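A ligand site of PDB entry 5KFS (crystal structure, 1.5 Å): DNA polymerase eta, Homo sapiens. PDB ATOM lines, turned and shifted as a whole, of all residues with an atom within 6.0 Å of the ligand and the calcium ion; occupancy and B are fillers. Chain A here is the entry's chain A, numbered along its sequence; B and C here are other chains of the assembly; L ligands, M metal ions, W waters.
Three residues have an atom within 4 Å of the calcium ion: Asp 16, Met 17 and Asp 118.
The nearest printed residue that does not touch the calcium ion is Lys 234 (4.02 Å).
The calcium ion is bound by the side-chain carboxylate (OD2) of Asp 16 (2.2 Å), the side-chain carboxylate (OD1) of Asp 118 (2.3 Å), an oxygen (O4) of the ligand (2.3 Å), the backbone carbonyl oxygen (O) of Met 17 (2.3 Å), an oxygen (O1) of the ligand (2.3 Å) and an oxygen (O7) of the ligand (2.4 Å).
The calcium ion has six donor atoms within binding distance.
The backbone NH (N) of Asp 118 sits close to the side-chain hydroxyl (OG) of Ser 116.
O of Met 17 sits close to NZ of Lys 234 (3.3 Å).
NH1 of Arg 58 sits at hydrogen-bond distance from OH of Tyr 55.
O2 of DT 4 of chain B lies within hydrogen-bond range of the side-chain amide nitrogen (NE2) of Gln 41 (2.7 Å).
The backbone carbonyl oxygen (O) of Val 53 lies within hydrogen-bond range of the guanidinium group (NE) of Arg 58 (2.9 Å).
The side-chain amino group (NZ) of Lys 234 is in salt-bridge range of the side-chain carboxylate (OD1) of Asp 18 (2.7 Å).
N1 of DA 5 of chain B sits close to N3 of DT 8 of chain C.
O3' of DT 8 of chain C is in hydrogen-bond range of the side-chain hydroxyl (OG) of Ser 116, 2.7 Å away.
Water W3 lies within hydrogen-bond range of O5 of the ligand (2.7 Å), N of Val 53 (2.8 Å) and NH2 of Arg 58 (2.9 Å).
Water W8 lies within hydrogen-bond range of O of Ile 51 and N2 of the ligand.
Water W9 lies within hydrogen-bond range of O2 of DT 8 of chain C (2.5 Å) and O11 of the ligand (3.0 Å).
N1 of DA 5 of chain B sits close to a nitrogen (N4) of the ligand (3.3 Å).
Asp 18 touches the ligand.
Ile 51 touches the ligand.
Ala 52 touches the ligand (CB to O12, 3.4 Å).
Ile 117 touches the ligand.
O4 of DT 3 of chain B touches N3 of the ligand, 3.6 Å away.
Hydrophobic or aromatic side chains within 4 Å of the ligand: Phe 20, Phe 21, Ala 52, Tyr 55 and Ile 117.
Of the 23 residues printed, 17 come within 4 Å of the ligand.
The nearest printed residue that does not touch the ligand is Val 53 (4.8 Å).
The side-chain hydroxyl (OH) of Tyr 55 sits at hydrogen-bond distance from an oxygen (O2) of the ligand (2.6 Å).
N3 of the ligand sits at hydrogen-bond distance from O4 of DT 4 of chain B (3.0 Å).
O2 of the ligand lies within hydrogen-bond range of N of Cys 19 (2.8 Å).
An oxygen (O3) of the ligand lies within salt-bridge range of the guanidinium group (NH1) of Arg 58 (3.2 Å).
O5 of the ligand lies within hydrogen-bond range of N of Phe 20, at 3.4 Å.
The backbone NH (N) of Phe 21 sits at hydrogen-bond distance from an oxygen (O12) of the ligand (3.1 Å).
The side-chain amino group (NZ) of Lys 234 is in salt-bridge range of an oxygen (O2) of the ligand (3.4 Å).
O4 of DT 8 of chain C is in hydrogen-bond range of N3 of the ligand (3.4 Å).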
ATOM      1  N   ASP A  16      -2.209  17.180   3.320  1.00  0.00           N
ATOM      2  CA  ASP A  16      -2.637  17.303   4.714  1.00  0.00           C
ATOM      3  C   ASP A  16      -1.900  18.488   5.322  1.00  0.00           C
ATOM      4  O   ASP A  16      -0.676  18.430   5.500  1.00  0.00           O
ATOM      5  CB  ASP A  16      -2.282  15.995   5.457  1.00  0.00           C
ATOM      6  CG  ASP A  16      -2.899  15.883   6.827  1.00  0.00           C
ATOM      7  OD1 ASP A  16      -3.014  14.730   7.328  1.00  0.00           O
ATOM      8  OD2 ASP A  16      -3.238  16.910   7.436  1.00  0.00           O
ATOM      9  N   MET A  17      -2.612  19.570   5.662  1.00  0.00           N
ATOM     10  CA  MET A  17      -1.975  20.744   6.251  1.00  0.00           C
ATOM     11  C   MET A  17      -1.298  20.382   7.592  1.00  0.00           C
ATOM     12  O   MET A  17      -1.784  19.633   8.340  1.00  0.00           O
ATOM     13  CB  MET A  17      -2.966  21.923   6.446  1.00  0.00           C
ATOM     14  CG  MET A  17      -3.787  22.280   5.214  1.00  0.00           C
ATOM     15  SD  MET A  17      -2.799  22.707   3.741  1.00  0.00           S
ATOM     16  CE  MET A  17      -1.981  24.163   4.299  1.00  0.00           C
ATOM     17  N   ASP A  18      -0.153  20.980   7.824  1.00  0.00           N
ATOM     18  CA  ASP A  18       0.544  20.706   9.075  1.00  0.00           C
ATOM     19  C   ASP A  18      -0.047  21.553  10.194  1.00  0.00           C
ATOM     20  O   ASP A  18      -0.324  22.694   9.975  1.00  0.00           O
ATOM     21  CB  ASP A  18       2.022  21.008   8.943  1.00  0.00           C
ATOM     22  CG  ASP A  18       2.725  20.127   7.922  1.00  0.00           C
ATOM     23  OD1 ASP A  18       2.370  19.012   7.761  1.00  0.00           O
ATOM     24  OD2 ASP A  18       3.626  20.637   7.389  1.00  0.00           O
ATOM     25  N   CYS A  19      -0.332  20.923  11.322  1.00  0.00           N
ATOM     26  CA  CYS A  19      -0.826  21.607  12.523  1.00  0.00           C
ATOM     27  C   CYS A  19      -1.821  22.730  12.195  1.00  0.00           C
ATOM     28  O   CYS A  19      -1.530  23.845  12.509  1.00  0.00           O
ATOM     29  CB  CYS A  19       0.243  21.954  13.550  1.00  0.00           C
ATOM     30  SG  CYS A  19       1.589  23.050  12.975  1.00  0.00           S
ATOM     31  N   PHE A  20      -2.886  22.446  11.484  1.00  0.00           N
ATOM     32  CA  PHE A  20      -3.564  23.437  10.702  1.00  0.00           C
ATOM     33  C   PHE A  20      -4.114  24.621  11.485  1.00  0.00           C
ATOM     34  O   PHE A  20      -3.798  25.716  11.149  1.00  0.00           O
ATOM     35  CB  PHE A  20      -4.695  22.811   9.890  1.00  0.00           C
ATOM     36  CG  PHE A  20      -5.376  23.782   8.961  1.00  0.00           C
ATOM     37  CD1 PHE A  20      -4.637  24.532   8.098  1.00  0.00           C
ATOM     38  CD2 PHE A  20      -6.740  23.966   8.944  1.00  0.00           C
ATOM     39  CE1 PHE A  20      -5.242  25.442   7.260  1.00  0.00           C
ATOM     40  CE2 PHE A  20      -7.340  24.869   8.060  1.00  0.00           C
ATOM     41  CZ  PHE A  20      -6.595  25.587   7.234  1.00  0.00           C
ATOM     42  N   PHE A  21      -4.828  24.385  12.550  1.00  0.00           N
ATOM     43  CA  PHE A  21      -5.388  25.553  13.245  1.00  0.00           C
ATOM     44  C   PHE A  21      -4.274  26.406  13.858  1.00  0.00           C
ATOM     45  O   PHE A  21      -4.419  27.613  13.962  1.00  0.00           O
ATOM     46  CB  PHE A  21      -6.373  25.152  14.346  1.00  0.00           C
ATOM     47  CG  PHE A  21      -7.688  24.603  13.868  1.00  0.00           C
ATOM     48  CD1 PHE A  21      -7.896  24.159  12.568  1.00  0.00           C
ATOM     49  CD2 PHE A  21      -8.726  24.493  14.767  1.00  0.00           C
ATOM     50  CE1 PHE A  21      -9.139  23.657  12.168  1.00  0.00           C
ATOM     51  CE2 PHE A  21      -9.966  23.975  14.386  1.00  0.00           C
ATOM     52  CZ  PHE A  21     -10.160  23.539  13.090  1.00  0.00           C
ATOM     53  N   VAL A  22      -3.178  25.762  14.279  1.00  0.00           N
ATOM     54  CA  VAL A  22      -2.023  26.498  14.784  1.00  0.00           C
ATOM     55  C   VAL A  22      -1.439  27.397  13.685  1.00  0.00           C
ATOM     56  O   VAL A  22      -1.157  28.579  13.949  1.00  0.00           O
ATOM     57  CB  VAL A  22      -0.936  25.555  15.335  1.00  0.00           C
ATOM     58  CG1 VAL A  22       0.407  26.261  15.452  1.00  0.00           C
ATOM     59  CG2 VAL A  22      -1.375  24.975  16.675  1.00  0.00           C
ATOM     60  N   GLN A  41      -9.911  25.460  22.984  1.00  0.00           N
ATOM     61  CA  GLN A  41     -11.277  25.957  22.968  1.00  0.00           C
ATOM     62  C   GLN A  41     -11.820  26.028  24.380  1.00  0.00           C
ATOM     63  O   GLN A  41     -11.667  25.076  25.147  1.00  0.00           O
ATOM     64  CB  GLN A  41     -12.187  25.105  22.069  1.00  0.00           C
ATOM     65  CG  GLN A  41     -12.065  23.611  22.199  1.00  0.00           C
ATOM     66  CD  GLN A  41     -12.922  22.892  21.161  1.00  0.00           C
ATOM     67  OE1 GLN A  41     -13.438  23.513  20.225  1.00  0.00           O
ATOM     68  NE2 GLN A  41     -13.096  21.597  21.336  1.00  0.00           N
ATOM     69  N   ILE A  51      -6.893  21.572  20.885  1.00  0.00           N
ATOM     70  CA  ILE A  51      -7.308  20.882  19.675  1.00  0.00           C
ATOM     71  C   ILE A  51      -6.273  20.905  18.541  1.00  0.00           C
ATOM     72  O   ILE A  51      -6.449  20.199  17.559  1.00  0.00           O
ATOM     73  CB  ILE A  51      -8.646  21.437  19.136  1.00  0.00           C
ATOM     74  CG1 ILE A  51      -8.553  22.933  18.751  1.00  0.00           C
ATOM     75  CG2 ILE A  51      -9.755  21.183  20.146  1.00  0.00           C
ATOM     76  CD1 ILE A  51      -9.805  23.443  18.027  1.00  0.00           C
ATOM     77  N   ALA A  52      -5.202  21.666  18.689  1.00  0.00           N
ATOM     78  CA  ALA A  52      -4.100  21.630  17.707  1.00  0.00           C
ATOM     79  C   ALA A  52      -2.793  22.062  18.373  1.00  0.00           C
ATOM     80  O   ALA A  52      -2.826  22.893  19.282  1.00  0.00           O
ATOM     81  CB  ALA A  52      -4.404  22.513  16.487  1.00  0.00           C
ATOM     82  N   VAL A  53      -1.664  21.500  17.937  1.00  0.00           N
ATOM     83  CA  VAL A  53      -0.377  21.657  18.619  1.00  0.00           C
ATOM     84  C   VAL A  53       0.773  21.821  17.627  1.00  0.00           C
ATOM     85  O   VAL A  53       0.914  20.996  16.715  1.00  0.00           O
ATOM     86  CB  VAL A  53      -0.075  20.436  19.534  1.00  0.00           C
ATOM     87  CG1 VAL A  53       1.186  20.660  20.349  1.00  0.00           C
ATOM     88  CG2 VAL A  53      -1.231  20.158  20.455  1.00  0.00           C
ATOM     89  N   TYR A  55       4.621  21.793  16.176  1.00  0.00           N
ATOM     90  CA  TYR A  55       5.609  20.725  16.280  1.00  0.00           C
ATOM     91  C   TYR A  55       6.644  21.024  17.370  1.00  0.00           C
ATOM     92  O   TYR A  55       7.113  20.095  18.046  1.00  0.00           O
ATOM     93  CB  TYR A  55       6.272  20.469  14.910  1.00  0.00           C
ATOM     94  CG  TYR A  55       5.359  19.629  14.043  1.00  0.00           C
ATOM     95  CD1 TYR A  55       4.268  20.187  13.382  1.00  0.00           C
ATOM     96  CD2 TYR A  55       5.504  18.251  13.987  1.00  0.00           C
ATOM     97  CE1 TYR A  55       3.392  19.419  12.654  1.00  0.00           C
ATOM     98  CE2 TYR A  55       4.641  17.473  13.258  1.00  0.00           C
ATOM     99  CZ  TYR A  55       3.581  18.051  12.593  1.00  0.00           C
ATOM    100  OH  TYR A  55       2.716  17.259  11.875  1.00  0.00           O
ATOM    101  N   ARG A  58       4.935  19.796  20.416  1.00  0.00           N
ATOM    102  CA  ARG A  58       4.865  18.337  20.457  1.00  0.00           C
ATOM    103  C   ARG A  58       6.152  17.727  21.017  1.00  0.00           C
ATOM    104  O   ARG A  58       6.108  16.670  21.639  1.00  0.00           O
ATOM    105  CB  ARG A  58       4.584  17.753  19.076  1.00  0.00           C
ATOM    106  CG  ARG A  58       3.263  18.203  18.502  1.00  0.00           C
ATOM    107  CD  ARG A  58       3.023  17.567  17.150  1.00  0.00           C
ATOM    108  NE  ARG A  58       1.938  18.254  16.475  1.00  0.00           N
ATOM    109  CZ  ARG A  58       1.313  17.818  15.391  1.00  0.00           C
ATOM    110  NH1 ARG A  58       1.667  16.658  14.843  1.00  0.00           N
ATOM    111  NH2 ARG A  58       0.328  18.546  14.848  1.00  0.00           N
ATOM    112  N   SER A 116     -11.469  16.458   4.714  1.00  0.00           N
ATOM    113  CA  SER A 116     -11.677  17.075   6.024  1.00  0.00           C
ATOM    114  C   SER A 116     -11.400  18.549   5.895  1.00  0.00           C
ATOM    115  O   SER A 116     -11.131  19.045   4.800  1.00  0.00           O
ATOM    116  CB  SER A 116     -10.759  16.473   7.076  1.00  0.00           C
ATOM    117  OG  SER A 116      -9.425  16.882   6.817  1.00  0.00           O
ATOM    118  N   ILE A 117     -11.402  19.261   7.028  1.00  0.00           N
ATOM    119  CA  ILE A 117     -11.153  20.695   6.971  1.00  0.00           C
ATOM    120  C   ILE A 117      -9.754  21.034   6.406  1.00  0.00           C
ATOM    121  O   ILE A 117      -9.562  22.104   5.856  1.00  0.00           O
ATOM    122  CB  ILE A 117     -11.336  21.335   8.375  1.00  0.00           C
ATOM    123  CG1 ILE A 117     -11.508  22.851   8.250  1.00  0.00           C
ATOM    124  CG2 ILE A 117     -10.211  20.920   9.291  1.00  0.00           C
ATOM    125  CD1 ILE A 117     -12.095  23.526   9.492  1.00  0.00           C
ATOM    126  N   ASP A 118      -8.796  20.106   6.500  1.00  0.00           N
ATOM    127  CA  ASP A 118      -7.435  20.434   6.051  1.00  0.00           C
ATOM    128  C   ASP A 118      -6.766  19.329   5.229  1.00  0.00           C
ATOM    129  O   ASP A 118      -5.549  19.316   5.076  1.00  0.00           O
ATOM    130  CB  ASP A 118      -6.562  20.791   7.257  1.00  0.00           C
ATOM    131  CG  ASP A 118      -6.055  19.572   7.991  1.00  0.00           C
ATOM    132  OD1 ASP A 118      -4.910  19.638   8.504  1.00  0.00           O
ATOM    133  OD2 ASP A 118      -6.773  18.553   8.021  1.00  0.00           O
ATOM    134  N   GLU A 119      -7.581  18.419   4.693  1.00  0.00           N
ATOM    135  CA  GLU A 119      -7.095  17.316   3.856  1.00  0.00           C
ATOM    136  C   GLU A 119      -7.852  17.250   2.566  1.00  0.00           C
ATOM    137  O   GLU A 119      -9.074  17.361   2.560  1.00  0.00           O
ATOM    138  CB  GLU A 119      -7.253  15.964   4.546  1.00  0.00           C
ATOM    139  CG  GLU A 119      -6.237  15.670   5.598  1.00  0.00           C
ATOM    140  CD  GLU A 119      -6.440  14.298   6.186  1.00  0.00           C
ATOM    141  OE1 GLU A 119      -7.576  13.994   6.589  1.00  0.00           O
ATOM    142  OE2 GLU A 119      -5.474  13.513   6.218  1.00  0.00           O
ATOM    143  N   LYS A 234       6.479  13.977   8.158  1.00  0.00           N
ATOM    144  CA  LYS A 234       5.685  15.182   8.445  1.00  0.00           C
ATOM    145  C   LYS A 234       6.546  15.836   9.421  1.00  0.00           C
ATOM    146  O   LYS A 234       7.185  15.125  10.142  1.00  0.00           O
ATOM    147  CB  LYS A 234       4.399  14.823   9.165  1.00  0.00           C
ATOM    148  CG  LYS A 234       3.115  14.899   8.402  1.00  0.00           C
ATOM    149  CD  LYS A 234       1.870  15.397   9.217  1.00  0.00           C
ATOM    150  CE  LYS A 234       0.628  15.697   8.390  1.00  0.00           C
ATOM    151  NZ  LYS A 234       0.380  17.157   8.111  1.00  0.00           N
ATOM    152  N   PRO A 235       6.654  17.142   9.468  1.00  0.00           N
ATOM    153  CA  PRO A 235       5.869  18.067   8.642  1.00  0.00           C
ATOM    154  C   PRO A 235       6.656  18.599   7.449  1.00  0.00           C
ATOM    155  O   PRO A 235       7.871  18.377   7.333  1.00  0.00           O
ATOM    156  CB  PRO A 235       5.574  19.194   9.615  1.00  0.00           C
ATOM    157  CG  PRO A 235       6.872  19.279  10.434  1.00  0.00           C
ATOM    158  CD  PRO A 235       7.377  17.857  10.543  1.00  0.00           C
ATOM    159  P    DT B   3     -12.978  13.877  30.084  1.00  0.00           P
ATOM    160  OP1  DT B   3     -13.466  12.783  30.942  1.00  0.00           O
ATOM    161  OP2  DT B   3     -11.547  14.240  30.073  1.00  0.00           O
ATOM    162  O5'  DT B   3     -13.426  13.566  28.581  1.00  0.00           O
ATOM    163  C5'  DT B   3     -12.707  14.133  27.491  1.00  0.00           C
ATOM    164  C4'  DT B   3     -13.096  15.587  27.291  1.00  0.00           C
ATOM    165  O4'  DT B   3     -12.135  16.210  26.398  1.00  0.00           O
ATOM    166  C3'  DT B   3     -14.458  15.805  26.659  1.00  0.00           C
ATOM    167  O3'  DT B   3     -15.044  17.003  27.150  1.00  0.00           O
ATOM    168  C2'  DT B   3     -14.119  15.921  25.177  1.00  0.00           C
ATOM    169  C1'  DT B   3     -12.799  16.675  25.238  1.00  0.00           C
ATOM    170  N1   DT B   3     -11.920  16.414  24.065  1.00  0.00           N
ATOM    171  C2   DT B   3     -11.409  17.479  23.336  1.00  0.00           C
ATOM    172  O2   DT B   3     -11.633  18.639  23.615  1.00  0.00           O
ATOM    173  N3   DT B   3     -10.619  17.116  22.276  1.00  0.00           N
ATOM    174  C4   DT B   3     -10.295  15.833  21.867  1.00  0.00           C
ATOM    175  O4   DT B   3      -9.577  15.615  20.896  1.00  0.00           O
ATOM    176  C5   DT B   3     -10.866  14.770  22.668  1.00  0.00           C
ATOM    177  C7   DT B   3     -10.580  13.334  22.329  1.00  0.00           C
ATOM    178  C6   DT B   3     -11.636  15.105  23.716  1.00  0.00           C
ATOM    179  P    DT B   4     -16.421  17.535  26.516  1.00  0.00           P
ATOM    180  OP1  DT B   4     -17.028  18.496  27.464  1.00  0.00           O
ATOM    181  OP2  DT B   4     -17.197  16.364  26.047  1.00  0.00           O
ATOM    182  O5'  DT B   4     -15.968  18.325  25.208  1.00  0.00           O
ATOM    183  C5'  DT B   4     -15.426  19.621  25.324  1.00  0.00           C
ATOM    184  C4'  DT B   4     -15.580  20.364  24.022  1.00  0.00           C
ATOM    185  O4'  DT B   4     -14.695  19.799  23.031  1.00  0.00           O
ATOM    186  C3'  DT B   4     -16.972  20.313  23.390  1.00  0.00           C
ATOM    187  O3'  DT B   4     -17.208  21.546  22.780  1.00  0.00           O
ATOM    188  C2'  DT B   4     -16.844  19.176  22.373  1.00  0.00           C
ATOM    189  C1'  DT B   4     -15.425  19.404  21.898  1.00  0.00           C
ATOM    190  N1   DT B   4     -14.743  18.222  21.301  1.00  0.00           N
ATOM    191  C2   DT B   4     -13.903  18.438  20.250  1.00  0.00           C
ATOM    192  O2   DT B   4     -13.732  19.532  19.764  1.00  0.00           O
ATOM    193  N3   DT B   4     -13.277  17.315  19.780  1.00  0.00           N
ATOM    194  C4   DT B   4     -13.384  16.027  20.244  1.00  0.00           C
ATOM    195  O4   DT B   4     -12.773  15.091  19.743  1.00  0.00           O
ATOM    196  C5   DT B   4     -14.273  15.862  21.376  1.00  0.00           C
ATOM    197  C7   DT B   4     -14.484  14.498  21.972  1.00  0.00           C
ATOM    198  C6   DT B   4     -14.897  16.960  21.861  1.00  0.00           C
ATOM    199  P    DA B   5     -18.577  21.858  22.003  1.00  0.00           P
ATOM    200  OP1  DA B   5     -18.920  23.256  22.308  1.00  0.00           O
ATOM    201  OP2  DA B   5     -19.543  20.774  22.227  1.00  0.00           O
ATOM    202  O5'  DA B   5     -18.148  21.758  20.460  1.00  0.00           O
ATOM    203  C5'  DA B   5     -17.237  22.688  19.914  1.00  0.00           C
ATOM    204  C4'  DA B   5     -17.054  22.433  18.442  1.00  0.00           C
ATOM    205  O4'  DA B   5     -16.295  21.214  18.243  1.00  0.00           O
ATOM    206  C3'  DA B   5     -18.356  22.257  17.649  1.00  0.00           C
ATOM    207  O3'  DA B   5     -18.223  22.904  16.381  1.00  0.00           O
ATOM    208  C2'  DA B   5     -18.439  20.734  17.484  1.00  0.00           C
ATOM    209  C1'  DA B   5     -16.964  20.418  17.295  1.00  0.00           C
ATOM    210  N9   DA B   5     -16.617  19.012  17.517  1.00  0.00           N
ATOM    211  C8   DA B   5     -17.132  18.174  18.466  1.00  0.00           C
ATOM    212  N7   DA B   5     -16.617  16.971  18.432  1.00  0.00           N
ATOM    213  C5   DA B   5     -15.707  17.014  17.388  1.00  0.00           C
ATOM    214  C6   DA B   5     -14.835  16.047  16.847  1.00  0.00           C
ATOM    215  N6   DA B   5     -14.752  14.792  17.307  1.00  0.00           N
ATOM    216  N1   DA B   5     -14.056  16.426  15.818  1.00  0.00           N
ATOM    217  C2   DA B   5     -14.147  17.680  15.363  1.00  0.00           C
ATOM    218  N3   DA B   5     -14.915  18.674  15.796  1.00  0.00           N
ATOM    219  C4   DA B   5     -15.690  18.263  16.824  1.00  0.00           C
ATOM    220  P    DT C   8      -7.725  10.862  10.861  1.00  0.00           P
ATOM    221  OP1  DT C   8      -6.501  10.764  10.037  1.00  0.00           O
ATOM    222  OP2  DT C   8      -7.641  10.639  12.322  1.00  0.00           O
ATOM    223  O5'  DT C   8      -8.439  12.307  10.671  1.00  0.00           O
ATOM    224  C5'  DT C   8      -8.332  13.019   9.433  1.00  0.00           C
ATOM    225  C4'  DT C   8      -9.018  14.385   9.508  1.00  0.00           C
ATOM    226  O4'  DT C   8     -10.208  14.288  10.319  1.00  0.00           O
ATOM    227  C3'  DT C   8      -8.197  15.538  10.106  1.00  0.00           C
ATOM    228  O3'  DT C   8      -8.382  16.699   9.342  1.00  0.00           O
ATOM    229  C2'  DT C   8      -8.759  15.696  11.510  1.00  0.00           C
ATOM    230  C1'  DT C   8     -10.213  15.302  11.307  1.00  0.00           C
ATOM    231  N1   DT C   8     -10.855  14.756  12.527  1.00  0.00           N
ATOM    232  C2   DT C   8     -11.776  15.531  13.199  1.00  0.00           C
ATOM    233  O2   DT C   8     -12.080  16.659  12.852  1.00  0.00           O
ATOM    234  N3   DT C   8     -12.322  14.928  14.314  1.00  0.00           N
ATOM    235  C4   DT C   8     -12.035  13.677  14.801  1.00  0.00           C
ATOM    236  O4   DT C   8     -12.581  13.229  15.812  1.00  0.00           O
ATOM    237  C5   DT C   8     -11.058  12.930  14.057  1.00  0.00           C
ATOM    238  C7   DT C   8     -10.690  11.541  14.504  1.00  0.00           C
ATOM    239  C6   DT C   8     -10.525  13.496  12.966  1.00  0.00           C
HETATM  240  P1  LIG L   1      -0.851  17.368  11.720  1.00  0.00           P
HETATM  241  O1  LIG L   1      -1.685  17.043  10.507  1.00  0.00           O
HETATM  242  O2  LIG L   1       0.342  18.185  11.338  1.00  0.00           O
HETATM  243  O3  LIG L   1      -0.427  16.142  12.527  1.00  0.00           O
HETATM  244  P2  LIG L   1      -3.167  18.884  12.581  1.00  0.00           P
HETATM  245  O4  LIG L   1      -3.338  19.473  11.202  1.00  0.00           O
HETATM  246  O5  LIG L   1      -3.366  19.877  13.710  1.00  0.00           O
HETATM  247  O6  LIG L   1      -1.683  18.263  12.753  1.00  0.00           O
HETATM  248  P3  LIG L   1      -5.292  17.039  11.958  1.00  0.00           P
HETATM  249  O7  LIG L   1      -4.851  16.895  10.560  1.00  0.00           O
HETATM  250  O8  LIG L   1      -5.688  15.751  12.643  1.00  0.00           O
HETATM  251  O9  LIG L   1      -4.129  17.652  12.846  1.00  0.00           O
HETATM  252  O10 LIG L   1      -6.538  17.997  12.093  1.00  0.00           O
HETATM  253  C1  LIG L   1      -6.664  19.190  11.385  1.00  0.00           C
HETATM  254  C2  LIG L   1      -7.283  20.259  12.287  1.00  0.00           C
HETATM  255  O11 LIG L   1      -8.593  19.820  12.609  1.00  0.00           O
HETATM  256  C3  LIG L   1      -6.568  20.461  13.550  1.00  0.00           C
HETATM  257  O12 LIG L   1      -5.569  21.487  13.411  1.00  0.00           O
HETATM  258  C4  LIG L   1      -7.635  20.838  14.501  1.00  0.00           C
HETATM  259  C5  LIG L   1      -8.832  20.114  13.993  1.00  0.00           C
HETATM  260  N1  LIG L   1      -9.106  18.896  14.673  1.00  0.00           N
HETATM  261  C6  LIG L   1      -8.545  17.681  14.456  1.00  0.00           C
HETATM  262  N2  LIG L   1      -9.055  16.767  15.273  1.00  0.00           N
HETATM  263  C7  LIG L   1      -9.991  17.368  16.042  1.00  0.00           C
HETATM  264  C8  LIG L   1     -10.850  16.956  17.056  1.00  0.00           C
HETATM  265  N3  LIG L   1     -10.867  15.603  17.508  1.00  0.00           N
HETATM  266  N4  LIG L   1     -11.653  17.849  17.624  1.00  0.00           N
HETATM  267  C9  LIG L   1     -11.695  19.140  17.248  1.00  0.00           C
HETATM  268  N5  LIG L   1     -10.873  19.579  16.258  1.00  0.00           N
HETATM  269  C10 LIG L   1     -10.034  18.713  15.659  1.00  0.00           C
HETATM  270 CA    CA M   1      -3.329  18.158   9.281  1.00  0.00          CA
HETATM  271  O   HOH W   1      -3.880  14.432   9.803  1.00  0.00           O
HETATM  272  O   HOH W   2     -12.326  21.719  15.237  1.00  0.00           O
HETATM  273  O   HOH W   3      -2.167  19.448  16.086  1.00  0.00           O
HETATM  274  O   HOH W   4      -3.807  13.843  13.726  1.00  0.00           O
HETATM  275  O   HOH W   5      -1.541  13.805  11.283  1.00  0.00           O
HETATM  276  O   HOH W   6      -5.338  16.170  15.894  1.00  0.00           O
HETATM  277  O   HOH W   7      -1.632  15.156  14.735  1.00  0.00           O
HETATM  278  O   HOH W   8      -7.243  17.606  17.352  1.00  0.00           O
HETATM  279  O   HOH W   9     -11.369  18.940  12.071  1.00  0.00           O
